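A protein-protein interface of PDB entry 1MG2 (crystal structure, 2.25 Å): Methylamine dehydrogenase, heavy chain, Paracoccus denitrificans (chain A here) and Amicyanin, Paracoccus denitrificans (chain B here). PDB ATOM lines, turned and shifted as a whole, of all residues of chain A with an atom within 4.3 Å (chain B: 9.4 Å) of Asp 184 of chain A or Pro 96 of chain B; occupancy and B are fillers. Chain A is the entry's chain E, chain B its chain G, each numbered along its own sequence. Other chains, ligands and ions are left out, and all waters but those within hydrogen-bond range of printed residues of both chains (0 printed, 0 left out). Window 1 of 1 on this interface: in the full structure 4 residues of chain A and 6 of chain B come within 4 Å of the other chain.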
ATOM      1  N   PHE A 160     -20.544 -22.553  11.336  1.00  0.00           N
ATOM      2  CA  PHE A 160     -20.913 -23.343  12.506  1.00  0.00           C
ATOM      3  C   PHE A 160     -22.390 -23.232  12.895  1.00  0.00           C
ATOM      4  O   PHE A 160     -23.078 -24.242  13.059  1.00  0.00           O
ATOM      5  CB  PHE A 160     -20.039 -22.930  13.697  1.00  0.00           C
ATOM      6  CG  PHE A 160     -20.372 -23.650  14.972  1.00  0.00           C
ATOM      7  CD1 PHE A 160     -20.017 -24.983  15.147  1.00  0.00           C
ATOM      8  CD2 PHE A 160     -21.069 -23.005  15.987  1.00  0.00           C
ATOM      9  CE1 PHE A 160     -20.354 -25.659  16.311  1.00  0.00           C
ATOM     10  CE2 PHE A 160     -21.412 -23.681  17.160  1.00  0.00           C
ATOM     11  CZ  PHE A 160     -21.052 -25.008  17.318  1.00  0.00           C
ATOM     12  N   PRO A 164     -24.277 -26.562  10.518  1.00  0.00           N
ATOM     13  CA  PRO A 164     -23.037 -26.828   9.790  1.00  0.00           C
ATOM     14  C   PRO A 164     -23.203 -26.661   8.284  1.00  0.00           C
ATOM     15  O   PRO A 164     -24.169 -27.144   7.695  1.00  0.00           O
ATOM     16  CB  PRO A 164     -22.698 -28.264  10.199  1.00  0.00           C
ATOM     17  CG  PRO A 164     -24.046 -28.867  10.451  1.00  0.00           C
ATOM     18  CD  PRO A 164     -24.738 -27.770  11.222  1.00  0.00           C
ATOM     19  N   VAL A 182     -24.064 -29.462   5.189  1.00  0.00           N
ATOM     20  CA  VAL A 182     -23.158 -30.555   5.497  1.00  0.00           C
ATOM     21  C   VAL A 182     -23.548 -31.229   6.816  1.00  0.00           C
ATOM     22  O   VAL A 182     -24.328 -30.678   7.585  1.00  0.00           O
ATOM     23  CB  VAL A 182     -21.714 -29.979   5.553  1.00  0.00           C
ATOM     24  CG1 VAL A 182     -20.849 -30.749   6.514  1.00  0.00           C
ATOM     25  CG2 VAL A 182     -21.109 -29.999   4.156  1.00  0.00           C
ATOM     26  N   PRO A 183     -23.043 -32.450   7.078  1.00  0.00           N
ATOM     27  CA  PRO A 183     -23.413 -33.089   8.345  1.00  0.00           C
ATOM     28  C   PRO A 183     -22.657 -32.385   9.469  1.00  0.00           C
ATOM     29  O   PRO A 183     -21.935 -31.421   9.222  1.00  0.00           O
ATOM     30  CB  PRO A 183     -22.937 -34.534   8.163  1.00  0.00           C
ATOM     31  CG  PRO A 183     -22.862 -34.714   6.678  1.00  0.00           C
ATOM     32  CD  PRO A 183     -22.318 -33.395   6.211  1.00  0.00           C
ATOM     33  N   ASP A 184     -22.814 -32.866  10.698  1.00  0.00           N
ATOM     34  CA  ASP A 184     -22.118 -32.263  11.828  1.00  0.00           C
ATOM     35  C   ASP A 184     -20.646 -32.632  11.748  1.00  0.00           C
ATOM     36  O   ASP A 184     -20.163 -33.491  12.477  1.00  0.00           O
ATOM     37  CB  ASP A 184     -22.719 -32.751  13.140  1.00  0.00           C
ATOM     38  CG  ASP A 184     -24.198 -32.442  13.244  1.00  0.00           C
ATOM     39  OD1 ASP A 184     -24.585 -31.282  12.983  1.00  0.00           O
ATOM     40  OD2 ASP A 184     -24.975 -33.355  13.589  1.00  0.00           O
ATOM     41  N   CYS A 185     -19.942 -31.966  10.847  1.00  0.00           N
ATOM     42  CA  CYS A 185     -18.526 -32.219  10.631  1.00  0.00           C
ATOM     43  C   CYS A 185     -17.786 -30.888  10.646  1.00  0.00           C
ATOM     44  O   CYS A 185     -18.404 -29.833  10.522  1.00  0.00           O
ATOM     45  CB  CYS A 185     -18.343 -32.935   9.297  1.00  0.00           C
ATOM     46  SG  CYS A 185     -19.530 -34.288   9.095  1.00  0.00           S
ATOM     47  N   TYR A 186     -16.463 -30.943  10.792  1.00  0.00           N
ATOM     48  CA  TYR A 186     -15.662 -29.735  10.885  1.00  0.00           C
ATOM     49  C   TYR A 186     -14.372 -29.801  10.075  1.00  0.00           C
ATOM     50  O   TYR A 186     -13.842 -30.886   9.824  1.00  0.00           O
ATOM     51  CB  TYR A 186     -15.360 -29.467  12.363  1.00  0.00           C
ATOM     52  CG  TYR A 186     -16.576 -29.665  13.246  1.00  0.00           C
ATOM     53  CD1 TYR A 186     -17.075 -30.948  13.500  1.00  0.00           C
ATOM     54  CD2 TYR A 186     -17.283 -28.573  13.753  1.00  0.00           C
ATOM     55  CE1 TYR A 186     -18.251 -31.137  14.223  1.00  0.00           C
ATOM     56  CE2 TYR A 186     -18.461 -28.757  14.481  1.00  0.00           C
ATOM     57  CZ  TYR A 186     -18.938 -30.041  14.702  1.00  0.00           C
ATOM     58  OH  TYR A 186     -20.128 -30.229  15.361  1.00  0.00           O
ATOM     59  N   CYS A 200     -15.940 -35.568  11.194  1.00  0.00           N
ATOM     60  CA  CYS A 200     -17.233 -35.529  11.871  1.00  0.00           C
ATOM     61  C   CYS A 200     -17.222 -35.827  13.356  1.00  0.00           C
ATOM     62  O   CYS A 200     -16.268 -36.390  13.888  1.00  0.00           O
ATOM     63  CB  CYS A 200     -18.195 -36.489  11.182  1.00  0.00           C
ATOM     64  SG  CYS A 200     -18.177 -36.319   9.405  1.00  0.00           S
ATOM     65  N   ARG A 201     -18.314 -35.449  14.015  1.00  0.00           N
ATOM     66  CA  ARG A 201     -18.466 -35.656  15.441  1.00  0.00           C
ATOM     67  C   ARG A 201     -18.358 -37.130  15.792  1.00  0.00           C
ATOM     68  O   ARG A 201     -17.794 -37.477  16.827  1.00  0.00           O
ATOM     69  CB  ARG A 201     -19.814 -35.107  15.925  1.00  0.00           C
ATOM     70  CG  ARG A 201     -20.014 -35.175  17.450  1.00  0.00           C
ATOM     71  CD  ARG A 201     -21.429 -34.773  17.858  1.00  0.00           C
ATOM     72  NE  ARG A 201     -21.687 -34.959  19.287  1.00  0.00           N
ATOM     73  CZ  ARG A 201     -21.223 -34.173  20.259  1.00  0.00           C
ATOM     74  NH1 ARG A 201     -21.521 -34.447  21.522  1.00  0.00           N
ATOM     75  NH2 ARG A 201     -20.469 -33.114  19.976  1.00  0.00           N
ATOM     76  N   MET B  28     -27.098 -34.779  25.780  1.00  0.00           N
ATOM     77  CA  MET B  28     -26.860 -34.074  24.528  1.00  0.00           C
ATOM     78  C   MET B  28     -27.872 -34.391  23.440  1.00  0.00           C
ATOM     79  O   MET B  28     -27.522 -34.478  22.262  1.00  0.00           O
ATOM     80  CB  MET B  28     -25.454 -34.387  24.008  1.00  0.00           C
ATOM     81  CG  MET B  28     -24.344 -34.048  24.992  1.00  0.00           C
ATOM     82  SD  MET B  28     -24.480 -32.363  25.607  1.00  0.00           S
ATOM     83  CE  MET B  28     -23.762 -31.456  24.244  1.00  0.00           C
ATOM     84  N   TYR B  30     -32.427 -34.362  22.307  1.00  0.00           N
ATOM     85  CA  TYR B  30     -33.831 -34.139  22.597  1.00  0.00           C
ATOM     86  C   TYR B  30     -34.371 -35.565  22.619  1.00  0.00           C
ATOM     87  O   TYR B  30     -34.361 -36.241  21.594  1.00  0.00           O
ATOM     88  CB  TYR B  30     -34.484 -33.335  21.473  1.00  0.00           C
ATOM     89  CG  TYR B  30     -33.946 -31.931  21.342  1.00  0.00           C
ATOM     90  CD1 TYR B  30     -34.186 -30.974  22.332  1.00  0.00           C
ATOM     91  CD2 TYR B  30     -33.192 -31.556  20.232  1.00  0.00           C
ATOM     92  CE1 TYR B  30     -33.688 -29.673  22.218  1.00  0.00           C
ATOM     93  CE2 TYR B  30     -32.690 -30.261  20.107  1.00  0.00           C
ATOM     94  CZ  TYR B  30     -32.943 -29.324  21.104  1.00  0.00           C
ATOM     95  OH  TYR B  30     -32.459 -28.044  20.971  1.00  0.00           O
ATOM     96  N   HIS B  53     -29.119 -26.090  27.676  1.00  0.00           N
ATOM     97  CA  HIS B  53     -29.666 -26.337  26.345  1.00  0.00           C
ATOM     98  C   HIS B  53     -30.820 -25.363  26.122  1.00  0.00           C
ATOM     99  O   HIS B  53     -31.343 -24.773  27.070  1.00  0.00           O
ATOM    100  CB  HIS B  53     -30.213 -27.766  26.230  1.00  0.00           C
ATOM    101  CG  HIS B  53     -29.180 -28.837  26.395  1.00  0.00           C
ATOM    102  ND1 HIS B  53     -28.196 -29.116  25.473  1.00  0.00           N
ATOM    103  CD2 HIS B  53     -29.005 -29.734  27.401  1.00  0.00           C
ATOM    104  CE1 HIS B  53     -27.471 -30.148  25.928  1.00  0.00           C
ATOM    105  NE2 HIS B  53     -27.922 -30.559  27.096  1.00  0.00           N
ATOM    106  N   ASN B  54     -31.219 -25.207  24.866  1.00  0.00           N
ATOM    107  CA  ASN B  54     -32.328 -24.329  24.502  1.00  0.00           C
ATOM    108  C   ASN B  54     -32.893 -24.892  23.206  1.00  0.00           C
ATOM    109  O   ASN B  54     -32.424 -25.916  22.708  1.00  0.00           O
ATOM    110  CB  ASN B  54     -31.825 -22.900  24.244  1.00  0.00           C
ATOM    111  CG  ASN B  54     -31.190 -22.736  22.854  1.00  0.00           C
ATOM    112  OD1 ASN B  54     -30.507 -23.636  22.359  1.00  0.00           O
ATOM    113  ND2 ASN B  54     -31.404 -21.578  22.231  1.00  0.00           N
ATOM    114  N   HIS B  56     -33.835 -23.669  19.270  1.00  0.00           N
ATOM    115  CA  HIS B  56     -33.563 -22.590  18.334  1.00  0.00           C
ATOM    116  C   HIS B  56     -34.199 -22.875  16.975  1.00  0.00           C
ATOM    117  O   HIS B  56     -33.872 -23.866  16.315  1.00  0.00           O
ATOM    118  CB  HIS B  56     -32.037 -22.425  18.214  1.00  0.00           C
ATOM    119  CG  HIS B  56     -31.592 -21.305  17.319  1.00  0.00           C
ATOM    120  ND1 HIS B  56     -30.279 -20.883  17.267  1.00  0.00           N
ATOM    121  CD2 HIS B  56     -32.267 -20.539  16.428  1.00  0.00           C
ATOM    122  CE1 HIS B  56     -30.164 -19.906  16.382  1.00  0.00           C
ATOM    123  NE2 HIS B  56     -31.357 -19.679  15.858  1.00  0.00           N
ATOM    124  N   TYR B  90     -35.854 -27.520  14.580  1.00  0.00           N
ATOM    125  CA  TYR B  90     -35.121 -26.696  15.532  1.00  0.00           C
ATOM    126  C   TYR B  90     -33.846 -27.395  15.957  1.00  0.00           C
ATOM    127  O   TYR B  90     -33.655 -28.580  15.680  1.00  0.00           O
ATOM    128  CB  TYR B  90     -35.964 -26.399  16.780  1.00  0.00           C
ATOM    129  CG  TYR B  90     -36.364 -27.614  17.598  1.00  0.00           C
ATOM    130  CD1 TYR B  90     -37.549 -28.301  17.324  1.00  0.00           C
ATOM    131  CD2 TYR B  90     -35.584 -28.046  18.676  1.00  0.00           C
ATOM    132  CE1 TYR B  90     -37.952 -29.382  18.107  1.00  0.00           C
ATOM    133  CE2 TYR B  90     -35.977 -29.125  19.463  1.00  0.00           C
ATOM    134  CZ  TYR B  90     -37.164 -29.786  19.178  1.00  0.00           C
ATOM    135  OH  TYR B  90     -37.581 -30.829  19.981  1.00  0.00           O
ATOM    136  N   HIS B  91     -32.975 -26.648  16.626  1.00  0.00           N
ATOM    137  CA  HIS B  91     -31.713 -27.185  17.107  1.00  0.00           C
ATOM    138  C   HIS B  91     -31.315 -26.414  18.360  1.00  0.00           C
ATOM    139  O   HIS B  91     -31.989 -25.463  18.757  1.00  0.00           O
ATOM    140  CB  HIS B  91     -30.622 -27.024  16.043  1.00  0.00           C
ATOM    141  CG  HIS B  91     -30.183 -25.606  15.842  1.00  0.00           C
ATOM    142  ND1 HIS B  91     -30.980 -24.658  15.238  1.00  0.00           N
ATOM    143  CD2 HIS B  91     -29.048 -24.965  16.209  1.00  0.00           C
ATOM    144  CE1 HIS B  91     -30.357 -23.493  15.243  1.00  0.00           C
ATOM    145  NE2 HIS B  91     -29.183 -23.652  15.828  1.00  0.00           N
ATOM    146  N   CYS B  92     -30.221 -26.828  18.983  1.00  0.00           N
ATOM    147  CA  CYS B  92     -29.730 -26.154  20.177  1.00  0.00           C
ATOM    148  C   CYS B  92     -28.602 -25.242  19.716  1.00  0.00           C
ATOM    149  O   CYS B  92     -27.629 -25.709  19.129  1.00  0.00           O
ATOM    150  CB  CYS B  92     -29.214 -27.173  21.189  1.00  0.00           C
ATOM    151  SG  CYS B  92     -28.654 -26.429  22.718  1.00  0.00           S
ATOM    152  N   THR B  93     -28.739 -23.950  19.989  1.00  0.00           N
ATOM    153  CA  THR B  93     -27.768 -22.947  19.558  1.00  0.00           C
ATOM    154  C   THR B  93     -26.280 -23.283  19.713  1.00  0.00           C
ATOM    155  O   THR B  93     -25.521 -23.192  18.750  1.00  0.00           O
ATOM    156  CB  THR B  93     -28.051 -21.584  20.228  1.00  0.00           C
ATOM    157  OG1 THR B  93     -29.364 -21.136  19.865  1.00  0.00           O
ATOM    158  CG2 THR B  93     -27.040 -20.558  19.770  1.00  0.00           C
ATOM    159  N   PRO B  94     -25.841 -23.664  20.920  1.00  0.00           N
ATOM    160  CA  PRO B  94     -24.417 -23.987  21.071  1.00  0.00           C
ATOM    161  C   PRO B  94     -24.060 -25.404  20.625  1.00  0.00           C
ATOM    162  O   PRO B  94     -22.890 -25.738  20.457  1.00  0.00           O
ATOM    163  CB  PRO B  94     -24.185 -23.781  22.564  1.00  0.00           C
ATOM    164  CG  PRO B  94     -25.502 -24.246  23.157  1.00  0.00           C
ATOM    165  CD  PRO B  94     -26.511 -23.592  22.234  1.00  0.00           C
ATOM    166  N   HIS B  95     -25.079 -26.233  20.437  1.00  0.00           N
ATOM    167  CA  HIS B  95     -24.887 -27.624  20.043  1.00  0.00           C
ATOM    168  C   HIS B  95     -25.700 -27.903  18.775  1.00  0.00           C
ATOM    169  O   HIS B  95     -26.719 -28.591  18.822  1.00  0.00           O
ATOM    170  CB  HIS B  95     -25.354 -28.531  21.188  1.00  0.00           C
ATOM    171  CG  HIS B  95     -24.824 -28.129  22.534  1.00  0.00           C
ATOM    172  ND1 HIS B  95     -25.534 -28.232  23.710  1.00  0.00           N
ATOM    173  CD2 HIS B  95     -23.622 -27.597  22.882  1.00  0.00           C
ATOM    174  CE1 HIS B  95     -24.768 -27.766  24.711  1.00  0.00           C
ATOM    175  NE2 HIS B  95     -23.595 -27.368  24.261  1.00  0.00           N
ATOM    176  N   PRO B  96     -25.251 -27.369  17.623  1.00  0.00           N
ATOM    177  CA  PRO B  96     -25.919 -27.536  16.327  1.00  0.00           C
ATOM    178  C   PRO B  96     -26.236 -28.982  15.979  1.00  0.00           C
ATOM    179  O   PRO B  96     -27.157 -29.240  15.208  1.00  0.00           O
ATOM    180  CB  PRO B  96     -24.934 -26.907  15.343  1.00  0.00           C
ATOM    181  CG  PRO B  96     -24.254 -25.869  16.165  1.00  0.00           C
ATOM    182  CD  PRO B  96     -24.017 -26.580  17.469  1.00  0.00           C
ATOM    183  N   PHE B  97     -25.476 -29.918  16.542  1.00  0.00           N
ATOM    184  CA  PHE B  97     -25.701 -31.333  16.278  1.00  0.00           C
ATOM    185  C   PHE B  97     -26.984 -31.813  16.944  1.00  0.00           C
ATOM    186  O   PHE B  97     -27.488 -32.893  16.633  1.00  0.00           O
ATOM    187  CB  PHE B  97     -24.517 -32.181  16.764  1.00  0.00           C
ATOM    188  CG  PHE B  97     -24.098 -31.893  18.178  1.00  0.00           C
ATOM    189  CD1 PHE B  97     -23.261 -30.822  18.464  1.00  0.00           C
ATOM    190  CD2 PHE B  97     -24.551 -32.686  19.224  1.00  0.00           C
ATOM    191  CE1 PHE B  97     -22.878 -30.543  19.774  1.00  0.00           C
ATOM    192  CE2 PHE B  97     -24.173 -32.415  20.540  1.00  0.00           C
ATOM    193  CZ  PHE B  97     -23.334 -31.340  20.814  1.00  0.00           C
ATOM    194  N   MET B  98     -27.501 -31.018  17.876  1.00  0.00           N
ATOM    195  CA  MET B  98     -28.748 -31.359  18.551  1.00  0.00           C
ATOM    196  C   MET B  98     -29.885 -30.804  17.708  1.00  0.00           C
ATOM    197  O   MET B  98     -30.044 -29.593  17.595  1.00  0.00           O
ATOM    198  CB  MET B  98     -28.802 -30.742  19.952  1.00  0.00           C
ATOM    199  CG  MET B  98     -27.989 -31.490  20.994  1.00  0.00           C
ATOM    200  SD  MET B  98     -28.041 -30.662  22.592  1.00  0.00           S
ATOM    201  CE  MET B  98     -29.667 -31.108  23.164  1.00  0.00           C
ATOM    202  N   ARG B  99     -30.667 -31.694  17.111  1.00  0.00           N
ATOM    203  CA  ARG B  99     -31.778 -31.279  16.268  1.00  0.00           C
ATOM    204  C   ARG B  99     -33.060 -32.023  16.608  1.00  0.00           C
ATOM    205  O   ARG B  99     -33.029 -33.146  17.105  1.00  0.00           O
ATOM    206  CB  ARG B  99     -31.425 -31.497  14.789  1.00  0.00           C
ATOM    207  CG  ARG B  99     -30.497 -30.426  14.206  1.00  0.00           C
ATOM    208  CD  ARG B  99     -30.139 -30.724  12.759  1.00  0.00           C
ATOM    209  NE  ARG B  99     -29.214 -31.846  12.667  1.00  0.00           N
ATOM    210  CZ  ARG B  99     -27.889 -31.731  12.671  1.00  0.00           C
ATOM    211  NH1 ARG B  99     -27.140 -32.823  12.593  1.00  0.00           N
ATOM    212  NH2 ARG B  99     -27.307 -30.535  12.725  1.00  0.00           N
ATOM    213  N   GLY B 100     -34.185 -31.371  16.345  1.00  0.00           N
ATOM    214  CA  GLY B 100     -35.481 -31.963  16.604  1.00  0.00           C
ATOM    215  C   GLY B 100     -36.510 -31.272  15.729  1.00  0.00           C
ATOM    216  O   GLY B 100     -36.181 -30.318  15.025  1.00  0.00           O
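Phe 160 of chain A touches Pro 94 of chain B (CZ to O, 3.7 Å).
Phe 160 of chain A touches Pro 96 of chain B.
Asp 184 of chain A touches Pro 96 of chain B.
Asp 184 of chain A touches Phe 97 of chain B.
CE2 of Phe 97 of chain B touches CZ of Arg 201 of chain A, at 3.4 Å.
N of Arg 201 of chain A sits at hydrogen-bond distance from O of Asp 184 of chain A (3.1 Å).
NH2 of Arg 99 of chain B is in hydrogen-bond range of O of Pro 96 of chain B.
SG of Cys 185 of chain A forms a disulfide with SG of Cys 200 of chain A (2.5 Å).
Of chain B, only Pro 96, Phe 97 and Arg 99 come within 4 Å of Asp 184 of chain A.
Printed residues of chain A within 4 Å of Pro 96 of chain B: Phe 160 (3.4 Å) and Asp 184 (3.97 Å).
No residue of chain B comes within 4 Å of Cys 185 of chain A.
No residue of chain B comes within 4 Å of Cys 200 of chain A.
Of the printed residues of chain B, Arg 201 of chain A touches Phe 97.
Of the printed residues of chain A, Phe 97 of chain B touches Asp 184 and Arg 201.
His 56 of chain B touches none of the printed residues of chain A.
The nearest residue of chain B that does not touch Asp 184 of chain A is Met 98 of chain B (5.5 Å).
The nearest residue of chain A that does not touch Pro 96 of chain B is Pro 164 of chain A (4.2 Å).
OD2 of Asp 184 of chain A is in salt-bridge range of NH1 of Arg 99 of chain B (2.4 Å).
Of the 9 printed residues of chain A, 3 touch a printed residue of chain B.
Hydrophobic or aromatic side chains of chain A that line the printed part of chain B: Phe 160.
Of the 16 printed residues of chain B, 4 touch a printed residue of chain A.
Hydrophobic or aromatic side chains of chain B within 4 Å of the printed part of chain A: Pro 96 and Phe 97.
Among the printed residues, 6 pairs touch across the chains.
Among the printed residues, Asp or Glu carboxylates within 4 Å of a Lys or Arg side-chain nitrogen of the other chain: Asp 184 of chain A with Arg 99 of chain B.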
